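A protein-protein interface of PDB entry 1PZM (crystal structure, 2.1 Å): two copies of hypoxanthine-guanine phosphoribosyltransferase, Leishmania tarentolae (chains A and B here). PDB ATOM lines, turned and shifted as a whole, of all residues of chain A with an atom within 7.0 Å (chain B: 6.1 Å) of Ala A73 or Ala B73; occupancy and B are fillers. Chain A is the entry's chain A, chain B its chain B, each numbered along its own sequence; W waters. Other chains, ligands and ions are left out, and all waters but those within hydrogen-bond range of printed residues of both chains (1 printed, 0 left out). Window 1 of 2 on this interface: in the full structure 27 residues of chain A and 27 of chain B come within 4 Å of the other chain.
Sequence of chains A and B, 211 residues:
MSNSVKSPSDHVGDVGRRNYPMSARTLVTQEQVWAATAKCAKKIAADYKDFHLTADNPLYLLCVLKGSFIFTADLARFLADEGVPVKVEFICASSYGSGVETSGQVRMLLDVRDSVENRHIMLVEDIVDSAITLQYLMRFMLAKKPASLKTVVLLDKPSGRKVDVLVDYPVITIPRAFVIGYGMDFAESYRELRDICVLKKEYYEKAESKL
Phe A69 touches Thr B72 (CE1 to CG2, 3.8 Å). CA of Ala B73 touches CE1 of Phe A69, at 3.7 Å. Ala B73 touches Ile A70 (CB to CG1, 3.7 Å). Arg B77 touches Ile A70. Thr A72 touches Phe B69. Ala A73 touches Phe B69 (CA to CE1, 3.6 Å). CB of Ala A73 touches CB of Ala B73, 3.6 Å away. Arg A77 touches Ile B70. Arg B77 touches Glu A192. Phe B78 touches Arg A194.
Water W1 lies within hydrogen-bond range of NH1 of Arg B77 and O of Arg A194.
The backbone carbonyl oxygen (O) of Ser A68 sits at hydrogen-bond distance from the side-chain hydroxyl (OG1) of Thr A72, at 2.8 Å. The guanidinium group of Arg B77 is in hydrogen-bond range of the backbone carbonyl oxygen of Ala B73, at 3.0 Å. O of Ser B68 is in hydrogen-bond range of OG1 of Thr B72 (2.9 Å). The side-chain carboxylate (OD1) of Asp B74 lies within salt-bridge range of the guanidinium group (NH2) of Arg B77, 2.9 Å away. The guanidinium group of Arg A77 lies within salt-bridge range of the side-chain carboxylate of Asp A74 (2.8 Å). O of Ala A73 sits at hydrogen-bond distance from NE of Arg A77.
Ala A73 touches three residues of chain B. Of chain A, only Phe A69 (3.7 Å), Ile A70 (3.7 Å) and Ala A73 (3.6 Å) come within 4 Å of Ala B73. Printed residues of chain B within 4 Å of Glu A192: Ala B76 and Arg B77. Of the printed residues of chain B, Asp A74 touches Arg B77. Printed residues of chain A within 4 Å of Phe B78: Arg A194 (3.4 Å). The nearest residue of chain B that does not touch Ala A73 is Arg B77 (5.1 Å). The nearest printed residue of chain A that does not touch Thr B72 is Ile A70 (5.9 Å).
OD2 of Asp A74 is in salt-bridge range of NH1 of Arg B77. The guanidinium group (NH1) of Arg A77 is in salt-bridge range of the side-chain carboxylate (OD2) of Asp B74.
Phe A69 touches Thr B72, and with the chains exchanged Thr A72 touches Phe B69. Ile A70 touches Ala B73, and with the chains exchanged Ala A73 touches Ile B70. Asp A74 touches Arg B77, and with the chains exchanged Arg A77 touches Asp B74. Arg B77 touches its own counterpart, Arg A77. 11 positions are printed for both chains.
Among the printed residues, 17 pairs touch across the chains.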
ATOM      1  N   LEU A  61     -18.952  -2.977 -35.050  1.00  0.00           N
ATOM      2  CA  LEU A  61     -18.011  -2.380 -34.089  1.00  0.00           C
ATOM      3  C   LEU A  61     -18.162  -3.184 -32.800  1.00  0.00           C
ATOM      4  O   LEU A  61     -19.283  -3.272 -32.247  1.00  0.00           O
ATOM      5  CB  LEU A  61     -18.339  -0.899 -33.848  1.00  0.00           C
ATOM      6  CG  LEU A  61     -18.217   0.063 -35.060  1.00  0.00           C
ATOM      7  CD1 LEU A  61     -18.700   1.456 -34.699  1.00  0.00           C
ATOM      8  CD2 LEU A  61     -16.793   0.108 -35.594  1.00  0.00           C
ATOM      9  N   CYS A  63     -17.284  -3.128 -29.182  1.00  0.00           N
ATOM     10  CA  CYS A  63     -16.847  -2.180 -28.157  1.00  0.00           C
ATOM     11  C   CYS A  63     -16.286  -2.891 -26.901  1.00  0.00           C
ATOM     12  O   CYS A  63     -16.982  -3.674 -26.255  1.00  0.00           O
ATOM     13  CB  CYS A  63     -17.994  -1.231 -27.781  1.00  0.00           C
ATOM     14  SG  CYS A  63     -17.723  -0.288 -26.284  1.00  0.00           S
ATOM     15  N   SER A  68     -13.911   1.747 -23.668  1.00  0.00           N
ATOM     16  CA  SER A  68     -14.080   2.145 -25.066  1.00  0.00           C
ATOM     17  C   SER A  68     -15.463   2.711 -25.340  1.00  0.00           C
ATOM     18  O   SER A  68     -15.741   3.082 -26.475  1.00  0.00           O
ATOM     19  CB  SER A  68     -13.803   0.977 -26.026  1.00  0.00           C
ATOM     20  OG  SER A  68     -12.635   0.274 -25.589  1.00  0.00           O
ATOM     21  N   PHE A  69     -16.340   2.747 -24.329  1.00  0.00           N
ATOM     22  CA  PHE A  69     -17.705   3.200 -24.653  1.00  0.00           C
ATOM     23  C   PHE A  69     -17.861   4.604 -25.228  1.00  0.00           C
ATOM     24  O   PHE A  69     -18.739   4.821 -26.107  1.00  0.00           O
ATOM     25  CB  PHE A  69     -18.738   2.943 -23.526  1.00  0.00           C
ATOM     26  CG  PHE A  69     -18.884   4.062 -22.512  1.00  0.00           C
ATOM     27  CD1 PHE A  69     -20.085   4.781 -22.436  1.00  0.00           C
ATOM     28  CD2 PHE A  69     -17.869   4.316 -21.557  1.00  0.00           C
ATOM     29  CE1 PHE A  69     -20.275   5.783 -21.450  1.00  0.00           C
ATOM     30  CE2 PHE A  69     -18.022   5.311 -20.590  1.00  0.00           C
ATOM     31  CZ  PHE A  69     -19.218   6.071 -20.555  1.00  0.00           C
ATOM     32  N   ILE A  70     -17.110   5.577 -24.731  1.00  0.00           N
ATOM     33  CA  ILE A  70     -17.230   6.912 -25.346  1.00  0.00           C
ATOM     34  C   ILE A  70     -16.681   7.007 -26.777  1.00  0.00           C
ATOM     35  O   ILE A  70     -17.344   7.532 -27.676  1.00  0.00           O
ATOM     36  CB  ILE A  70     -16.695   8.009 -24.413  1.00  0.00           C
ATOM     37  CG1 ILE A  70     -17.674   8.081 -23.199  1.00  0.00           C
ATOM     38  CG2 ILE A  70     -16.604   9.401 -25.183  1.00  0.00           C
ATOM     39  CD1 ILE A  70     -17.254   8.891 -22.012  1.00  0.00           C
ATOM     40  N   PHE A  71     -15.499   6.430 -26.978  1.00  0.00           N
ATOM     41  CA  PHE A  71     -14.854   6.384 -28.290  1.00  0.00           C
ATOM     42  C   PHE A  71     -15.767   5.677 -29.279  1.00  0.00           C
ATOM     43  O   PHE A  71     -15.913   6.130 -30.405  1.00  0.00           O
ATOM     44  CB  PHE A  71     -13.493   5.668 -28.162  1.00  0.00           C
ATOM     45  CG  PHE A  71     -12.729   5.569 -29.469  1.00  0.00           C
ATOM     46  CD1 PHE A  71     -12.581   6.681 -30.307  1.00  0.00           C
ATOM     47  CD2 PHE A  71     -12.098   4.357 -29.811  1.00  0.00           C
ATOM     48  CE1 PHE A  71     -11.894   6.574 -31.508  1.00  0.00           C
ATOM     49  CE2 PHE A  71     -11.337   4.266 -31.011  1.00  0.00           C
ATOM     50  CZ  PHE A  71     -11.257   5.355 -31.852  1.00  0.00           C
ATOM     51  N   THR A  72     -16.373   4.555 -28.850  1.00  0.00           N
ATOM     52  CA  THR A  72     -17.299   3.827 -29.700  1.00  0.00           C
ATOM     53  C   THR A  72     -18.527   4.731 -30.119  1.00  0.00           C
ATOM     54  O   THR A  72     -18.949   4.754 -31.278  1.00  0.00           O
ATOM     55  CB  THR A  72     -17.835   2.532 -28.979  1.00  0.00           C
ATOM     56  OG1 THR A  72     -16.752   1.612 -28.689  1.00  0.00           O
ATOM     57  CG2 THR A  72     -18.682   1.777 -29.943  1.00  0.00           C
ATOM     58  N   ALA A  73     -19.135   5.410 -29.145  1.00  0.00           N
ATOM     59  CA  ALA A  73     -20.290   6.275 -29.419  1.00  0.00           C
ATOM     60  C   ALA A  73     -19.938   7.324 -30.448  1.00  0.00           C
ATOM     61  O   ALA A  73     -20.768   7.645 -31.307  1.00  0.00           O
ATOM     62  CB  ALA A  73     -20.732   6.962 -28.150  1.00  0.00           C
ATOM     63  N   ASP A  74     -18.737   7.901 -30.319  1.00  0.00           N
ATOM     64  CA  ASP A  74     -18.342   9.014 -31.208  1.00  0.00           C
ATOM     65  C   ASP A  74     -17.854   8.454 -32.580  1.00  0.00           C
ATOM     66  O   ASP A  74     -18.239   8.927 -33.622  1.00  0.00           O
ATOM     67  CB  ASP A  74     -17.198   9.798 -30.533  1.00  0.00           C
ATOM     68  CG  ASP A  74     -17.679  10.662 -29.356  1.00  0.00           C
ATOM     69  OD1 ASP A  74     -18.917  10.635 -29.011  1.00  0.00           O
ATOM     70  OD2 ASP A  74     -16.864  11.407 -28.724  1.00  0.00           O
ATOM     71  N   LEU A  75     -17.034   7.404 -32.560  1.00  0.00           N
ATOM     72  CA  LEU A  75     -16.585   6.779 -33.818  1.00  0.00           C
ATOM     73  C   LEU A  75     -17.778   6.289 -34.622  1.00  0.00           C
ATOM     74  O   LEU A  75     -17.776   6.456 -35.836  1.00  0.00           O
ATOM     75  CB  LEU A  75     -15.630   5.614 -33.565  1.00  0.00           C
ATOM     76  CG  LEU A  75     -15.212   4.743 -34.753  1.00  0.00           C
ATOM     77  CD1 LEU A  75     -14.333   5.470 -35.869  1.00  0.00           C
ATOM     78  CD2 LEU A  75     -14.464   3.424 -34.220  1.00  0.00           C
ATOM     79  N   ALA A  76     -18.769   5.650 -33.958  1.00  0.00           N
ATOM     80  CA  ALA A  76     -19.995   5.253 -34.672  1.00  0.00           C
ATOM     81  C   ALA A  76     -20.607   6.402 -35.483  1.00  0.00           C
ATOM     82  O   ALA A  76     -20.964   6.215 -36.636  1.00  0.00           O
ATOM     83  CB  ALA A  76     -21.096   4.613 -33.739  1.00  0.00           C
ATOM     84  N   ARG A  77     -20.725   7.576 -34.866  1.00  0.00           N
ATOM     85  CA  ARG A  77     -21.286   8.750 -35.546  1.00  0.00           C
ATOM     86  C   ARG A  77     -20.415   9.357 -36.673  1.00  0.00           C
ATOM     87  O   ARG A  77     -20.919   9.745 -37.699  1.00  0.00           O
ATOM     88  CB  ARG A  77     -21.709   9.802 -34.526  1.00  0.00           C
ATOM     89  CG  ARG A  77     -22.911   9.340 -33.663  1.00  0.00           C
ATOM     90  CD  ARG A  77     -23.203  10.267 -32.529  1.00  0.00           C
ATOM     91  NE  ARG A  77     -22.294  10.118 -31.385  1.00  0.00           N
ATOM     92  CZ  ARG A  77     -22.562  10.760 -30.232  1.00  0.00           C
ATOM     93  NH1 ARG A  77     -23.717  11.525 -30.122  1.00  0.00           N
ATOM     94  NH2 ARG A  77     -21.747  10.647 -29.195  1.00  0.00           N
ATOM     95  N   PHE A  78     -19.110   9.400 -36.502  1.00  0.00           N
ATOM     96  CA  PHE A  78     -18.212   9.714 -37.619  1.00  0.00           C
ATOM     97  C   PHE A  78     -18.302   8.736 -38.810  1.00  0.00           C
ATOM     98  O   PHE A  78     -18.224   9.146 -39.986  1.00  0.00           O
ATOM     99  CB  PHE A  78     -16.741   9.842 -37.111  1.00  0.00           C
ATOM    100  CG  PHE A  78     -16.528  11.066 -36.256  1.00  0.00           C
ATOM    101  CD1 PHE A  78     -16.100  10.939 -34.938  1.00  0.00           C
ATOM    102  CD2 PHE A  78     -16.845  12.344 -36.767  1.00  0.00           C
ATOM    103  CE1 PHE A  78     -15.969  12.093 -34.120  1.00  0.00           C
ATOM    104  CE2 PHE A  78     -16.745  13.494 -35.980  1.00  0.00           C
ATOM    105  CZ  PHE A  78     -16.295  13.365 -34.626  1.00  0.00           C
ATOM    106  N   VAL A 124     -12.829  -2.369 -31.040  1.00  0.00           N
ATOM    107  CA  VAL A 124     -12.729  -0.947 -30.745  1.00  0.00           C
ATOM    108  C   VAL A 124     -12.173  -0.813 -29.323  1.00  0.00           C
ATOM    109  O   VAL A 124     -12.769  -1.261 -28.368  1.00  0.00           O
ATOM    110  CB  VAL A 124     -14.105  -0.204 -30.835  1.00  0.00           C
ATOM    111  CG1 VAL A 124     -13.919   1.275 -30.414  1.00  0.00           C
ATOM    112  CG2 VAL A 124     -14.692  -0.290 -32.261  1.00  0.00           C
ATOM    113  N   TYR A 182     -12.384  10.773 -21.265  1.00  0.00           N
ATOM    114  CA  TYR A 182     -12.825  10.201 -22.559  1.00  0.00           C
ATOM    115  C   TYR A 182     -13.065   8.641 -22.469  1.00  0.00           C
ATOM    116  O   TYR A 182     -12.721   7.833 -23.386  1.00  0.00           O
ATOM    117  CB  TYR A 182     -11.895  10.657 -23.694  1.00  0.00           C
ATOM    118  CG  TYR A 182     -12.539  10.555 -25.063  1.00  0.00           C
ATOM    119  CD1 TYR A 182     -13.409  11.559 -25.515  1.00  0.00           C
ATOM    120  CD2 TYR A 182     -12.317   9.435 -25.872  1.00  0.00           C
ATOM    121  CE1 TYR A 182     -14.066  11.436 -26.726  1.00  0.00           C
ATOM    122  CE2 TYR A 182     -12.957   9.302 -27.098  1.00  0.00           C
ATOM    123  CZ  TYR A 182     -13.817  10.324 -27.522  1.00  0.00           C
ATOM    124  OH  TYR A 182     -14.443  10.234 -28.761  1.00  0.00           O
ATOM    125  N   ARG A 191     -13.874   8.771 -16.020  1.00  0.00           N
ATOM    126  CA  ARG A 191     -14.299   8.388 -17.381  1.00  0.00           C
ATOM    127  C   ARG A 191     -15.097   9.468 -18.089  1.00  0.00           C
ATOM    128  O   ARG A 191     -15.113   9.503 -19.305  1.00  0.00           O
ATOM    129  CB  ARG A 191     -15.270   7.187 -17.337  1.00  0.00           C
ATOM    130  CG  ARG A 191     -14.603   5.876 -16.813  1.00  0.00           C
ATOM    131  CD  ARG A 191     -15.503   4.675 -17.063  1.00  0.00           C
ATOM    132  NE  ARG A 191     -15.016   3.525 -16.326  1.00  0.00           N
ATOM    133  CZ  ARG A 191     -14.010   2.728 -16.707  1.00  0.00           C
ATOM    134  NH1 ARG A 191     -13.348   2.932 -17.855  1.00  0.00           N
ATOM    135  NH2 ARG A 191     -13.663   1.705 -15.945  1.00  0.00           N
ATOM    136  N   GLU A 192     -15.829  10.259 -17.299  1.00  0.00           N
ATOM    137  CA  GLU A 192     -16.705  11.322 -17.871  1.00  0.00           C
ATOM    138  C   GLU A 192     -16.011  12.590 -18.407  1.00  0.00           C
ATOM    139  O   GLU A 192     -16.640  13.473 -19.098  1.00  0.00           O
ATOM    140  CB  GLU A 192     -17.799  11.664 -16.824  1.00  0.00           C
ATOM    141  CG  GLU A 192     -17.362  12.522 -15.655  1.00  0.00           C
ATOM    142  CD  GLU A 192     -16.675  11.797 -14.497  1.00  0.00           C
ATOM    143  OE1 GLU A 192     -16.083  10.718 -14.734  1.00  0.00           O
ATOM    144  OE2 GLU A 192     -16.672  12.333 -13.353  1.00  0.00           O
ATOM    145  N   ARG A 194     -14.179  15.216 -20.626  1.00  0.00           N
ATOM    146  CA  ARG A 194     -14.228  15.401 -22.085  1.00  0.00           C
ATOM    147  C   ARG A 194     -12.870  15.317 -22.733  1.00  0.00           C
ATOM    148  O   ARG A 194     -12.756  14.898 -23.905  1.00  0.00           O
ATOM    149  CB  ARG A 194     -14.822  16.776 -22.428  1.00  0.00           C
ATOM    150  CG  ARG A 194     -16.302  16.926 -22.090  1.00  0.00           C
ATOM    151  CD  ARG A 194     -16.869  18.326 -22.563  1.00  0.00           C
ATOM    152  NE  ARG A 194     -18.311  18.406 -22.386  1.00  0.00           N
ATOM    153  CZ  ARG A 194     -19.217  17.954 -23.248  1.00  0.00           C
ATOM    154  NH1 ARG A 194     -18.836  17.347 -24.381  1.00  0.00           N
ATOM    155  NH2 ARG A 194     -20.544  18.123 -22.979  1.00  0.00           N
ATOM    156  N   SER B  68     -28.944   2.492 -24.864  1.00  0.00           N
ATOM    157  CA  SER B  68     -28.676   3.787 -24.224  1.00  0.00           C
ATOM    158  C   SER B  68     -27.218   4.175 -24.291  1.00  0.00           C
ATOM    159  O   SER B  68     -26.844   5.156 -23.670  1.00  0.00           O
ATOM    160  CB  SER B  68     -29.185   3.780 -22.755  1.00  0.00           C
ATOM    161  OG  SER B  68     -28.238   3.079 -21.989  1.00  0.00           O
ATOM    162  N   PHE B  69     -26.366   3.394 -24.992  1.00  0.00           N
ATOM    163  CA  PHE B  69     -24.918   3.649 -24.933  1.00  0.00           C
ATOM    164  C   PHE B  69     -24.481   5.068 -25.420  1.00  0.00           C
ATOM    165  O   PHE B  69     -23.507   5.644 -24.881  1.00  0.00           O
ATOM    166  CB  PHE B  69     -24.118   2.549 -25.624  1.00  0.00           C
ATOM    167  CG  PHE B  69     -23.814   2.748 -27.114  1.00  0.00           C
ATOM    168  CD1 PHE B  69     -22.508   3.091 -27.541  1.00  0.00           C
ATOM    169  CD2 PHE B  69     -24.770   2.497 -28.103  1.00  0.00           C
ATOM    170  CE1 PHE B  69     -22.152   3.181 -28.898  1.00  0.00           C
ATOM    171  CE2 PHE B  69     -24.399   2.621 -29.501  1.00  0.00           C
ATOM    172  CZ  PHE B  69     -23.100   2.943 -29.878  1.00  0.00           C
ATOM    173  N   ILE B  70     -25.154   5.600 -26.449  1.00  0.00           N
ATOM    174  CA  ILE B  70     -24.710   6.903 -26.925  1.00  0.00           C
ATOM    175  C   ILE B  70     -25.214   8.013 -25.995  1.00  0.00           C
ATOM    176  O   ILE B  70     -24.487   8.975 -25.668  1.00  0.00           O
ATOM    177  CB  ILE B  70     -25.119   7.120 -28.397  1.00  0.00           C
ATOM    178  CG1 ILE B  70     -24.250   6.236 -29.294  1.00  0.00           C
ATOM    179  CG2 ILE B  70     -25.035   8.657 -28.793  1.00  0.00           C
ATOM    180  CD1 ILE B  70     -24.572   6.320 -30.756  1.00  0.00           C
ATOM    181  N   PHE B  71     -26.475   7.873 -25.590  1.00  0.00           N
ATOM    182  CA  PHE B  71     -27.089   8.806 -24.626  1.00  0.00           C
ATOM    183  C   PHE B  71     -26.206   8.804 -23.343  1.00  0.00           C
ATOM    184  O   PHE B  71     -25.866   9.859 -22.806  1.00  0.00           O
ATOM    185  CB  PHE B  71     -28.566   8.358 -24.310  1.00  0.00           C
ATOM    186  CG  PHE B  71     -29.286   9.218 -23.258  1.00  0.00           C
ATOM    187  CD1 PHE B  71     -29.286  10.594 -23.352  1.00  0.00           C
ATOM    188  CD2 PHE B  71     -29.970   8.626 -22.206  1.00  0.00           C
ATOM    189  CE1 PHE B  71     -29.981  11.381 -22.403  1.00  0.00           C
ATOM    190  CE2 PHE B  71     -30.690   9.410 -21.286  1.00  0.00           C
ATOM    191  CZ  PHE B  71     -30.632  10.785 -21.371  1.00  0.00           C
ATOM    192  N   THR B  72     -25.763   7.634 -22.892  1.00  0.00           N
ATOM    193  CA  THR B  72     -24.924   7.609 -21.705  1.00  0.00           C
ATOM    194  C   THR B  72     -23.566   8.317 -21.941  1.00  0.00           C
ATOM    195  O   THR B  72     -23.101   9.031 -21.074  1.00  0.00           O
ATOM    196  CB  THR B  72     -24.623   6.123 -21.295  1.00  0.00           C
ATOM    197  OG1 THR B  72     -25.855   5.451 -20.980  1.00  0.00           O
ATOM    198  CG2 THR B  72     -23.776   6.037 -19.995  1.00  0.00           C
ATOM    199  N   ALA B  73     -22.915   8.076 -23.070  1.00  0.00           N
ATOM    200  CA  ALA B  73     -21.622   8.706 -23.358  1.00  0.00           C
ATOM    201  C   ALA B  73     -21.808  10.231 -23.352  1.00  0.00           C
ATOM    202  O   ALA B  73     -20.930  10.964 -22.872  1.00  0.00           O
ATOM    203  CB  ALA B  73     -21.068   8.248 -24.754  1.00  0.00           C
ATOM    204  N   ASP B  74     -22.956  10.705 -23.863  1.00  0.00           N
ATOM    205  CA  ASP B  74     -23.122  12.151 -23.997  1.00  0.00           C
ATOM    206  C   ASP B  74     -23.521  12.759 -22.653  1.00  0.00           C
ATOM    207  O   ASP B  74     -22.965  13.766 -22.238  1.00  0.00           O
ATOM    208  CB  ASP B  74     -24.195  12.512 -25.058  1.00  0.00           C
ATOM    209  CG  ASP B  74     -23.680  12.271 -26.502  1.00  0.00           C
ATOM    210  OD1 ASP B  74     -22.486  11.869 -26.683  1.00  0.00           O
ATOM    211  OD2 ASP B  74     -24.405  12.434 -27.506  1.00  0.00           O
ATOM    212  N   LEU B  75     -24.486  12.129 -21.988  1.00  0.00           N
ATOM    213  CA  LEU B  75     -24.974  12.617 -20.695  1.00  0.00           C
ATOM    214  C   LEU B  75     -23.823  12.634 -19.662  1.00  0.00           C
ATOM    215  O   LEU B  75     -23.707  13.610 -18.910  1.00  0.00           O
ATOM    216  CB  LEU B  75     -26.097  11.671 -20.168  1.00  0.00           C
ATOM    217  CG  LEU B  75     -26.513  11.768 -18.682  1.00  0.00           C
ATOM    218  CD1 LEU B  75     -27.164  13.156 -18.474  1.00  0.00           C
ATOM    219  CD2 LEU B  75     -27.485  10.618 -18.274  1.00  0.00           C
ATOM    220  N   ALA B  76     -22.955  11.601 -19.675  1.00  0.00           N
ATOM    221  CA  ALA B  76     -21.791  11.573 -18.777  1.00  0.00           C
ATOM    222  C   ALA B  76     -20.972  12.857 -18.912  1.00  0.00           C
ATOM    223  O   ALA B  76     -20.550  13.444 -17.898  1.00  0.00           O
ATOM    224  CB  ALA B  76     -20.854  10.353 -19.106  1.00  0.00           C
ATOM    225  N   ARG B  77     -20.798  13.316 -20.154  1.00  0.00           N
ATOM    226  CA  ARG B  77     -19.962  14.496 -20.417  1.00  0.00           C
ATOM    227  C   ARG B  77     -20.682  15.777 -20.043  1.00  0.00           C
ATOM    228  O   ARG B  77     -20.029  16.732 -19.666  1.00  0.00           O
ATOM    229  CB  ARG B  77     -19.492  14.525 -21.880  1.00  0.00           C
ATOM    230  CG  ARG B  77     -18.411  13.440 -22.108  1.00  0.00           C
ATOM    231  CD  ARG B  77     -17.888  13.291 -23.532  1.00  0.00           C
ATOM    232  NE  ARG B  77     -18.881  12.566 -24.347  1.00  0.00           N
ATOM    233  CZ  ARG B  77     -18.673  12.217 -25.603  1.00  0.00           C
ATOM    234  NH1 ARG B  77     -17.496  12.493 -26.180  1.00  0.00           N
ATOM    235  NH2 ARG B  77     -19.628  11.574 -26.287  1.00  0.00           N
ATOM    236  N   PHE B  78     -22.014  15.810 -20.159  1.00  0.00           N
ATOM    237  CA  PHE B  78     -22.765  16.991 -19.681  1.00  0.00           C
ATOM    238  C   PHE B  78     -22.720  17.016 -18.157  1.00  0.00           C
ATOM    239  O   PHE B  78     -22.667  18.091 -17.561  1.00  0.00           O
ATOM    240  CB  PHE B  78     -24.204  16.982 -20.211  1.00  0.00           C
ATOM    241  CG  PHE B  78     -24.301  17.313 -21.729  1.00  0.00           C
ATOM    242  CD1 PHE B  78     -24.797  16.381 -22.654  1.00  0.00           C
ATOM    243  CD2 PHE B  78     -23.808  18.527 -22.224  1.00  0.00           C
ATOM    244  CE1 PHE B  78     -24.823  16.704 -24.053  1.00  0.00           C
ATOM    245  CE2 PHE B  78     -23.853  18.833 -23.613  1.00  0.00           C
ATOM    246  CZ  PHE B  78     -24.346  17.951 -24.515  1.00  0.00           C
HETATM  247  O   HOH W   1     -15.385  14.359 -25.262  1.00  0.00           O
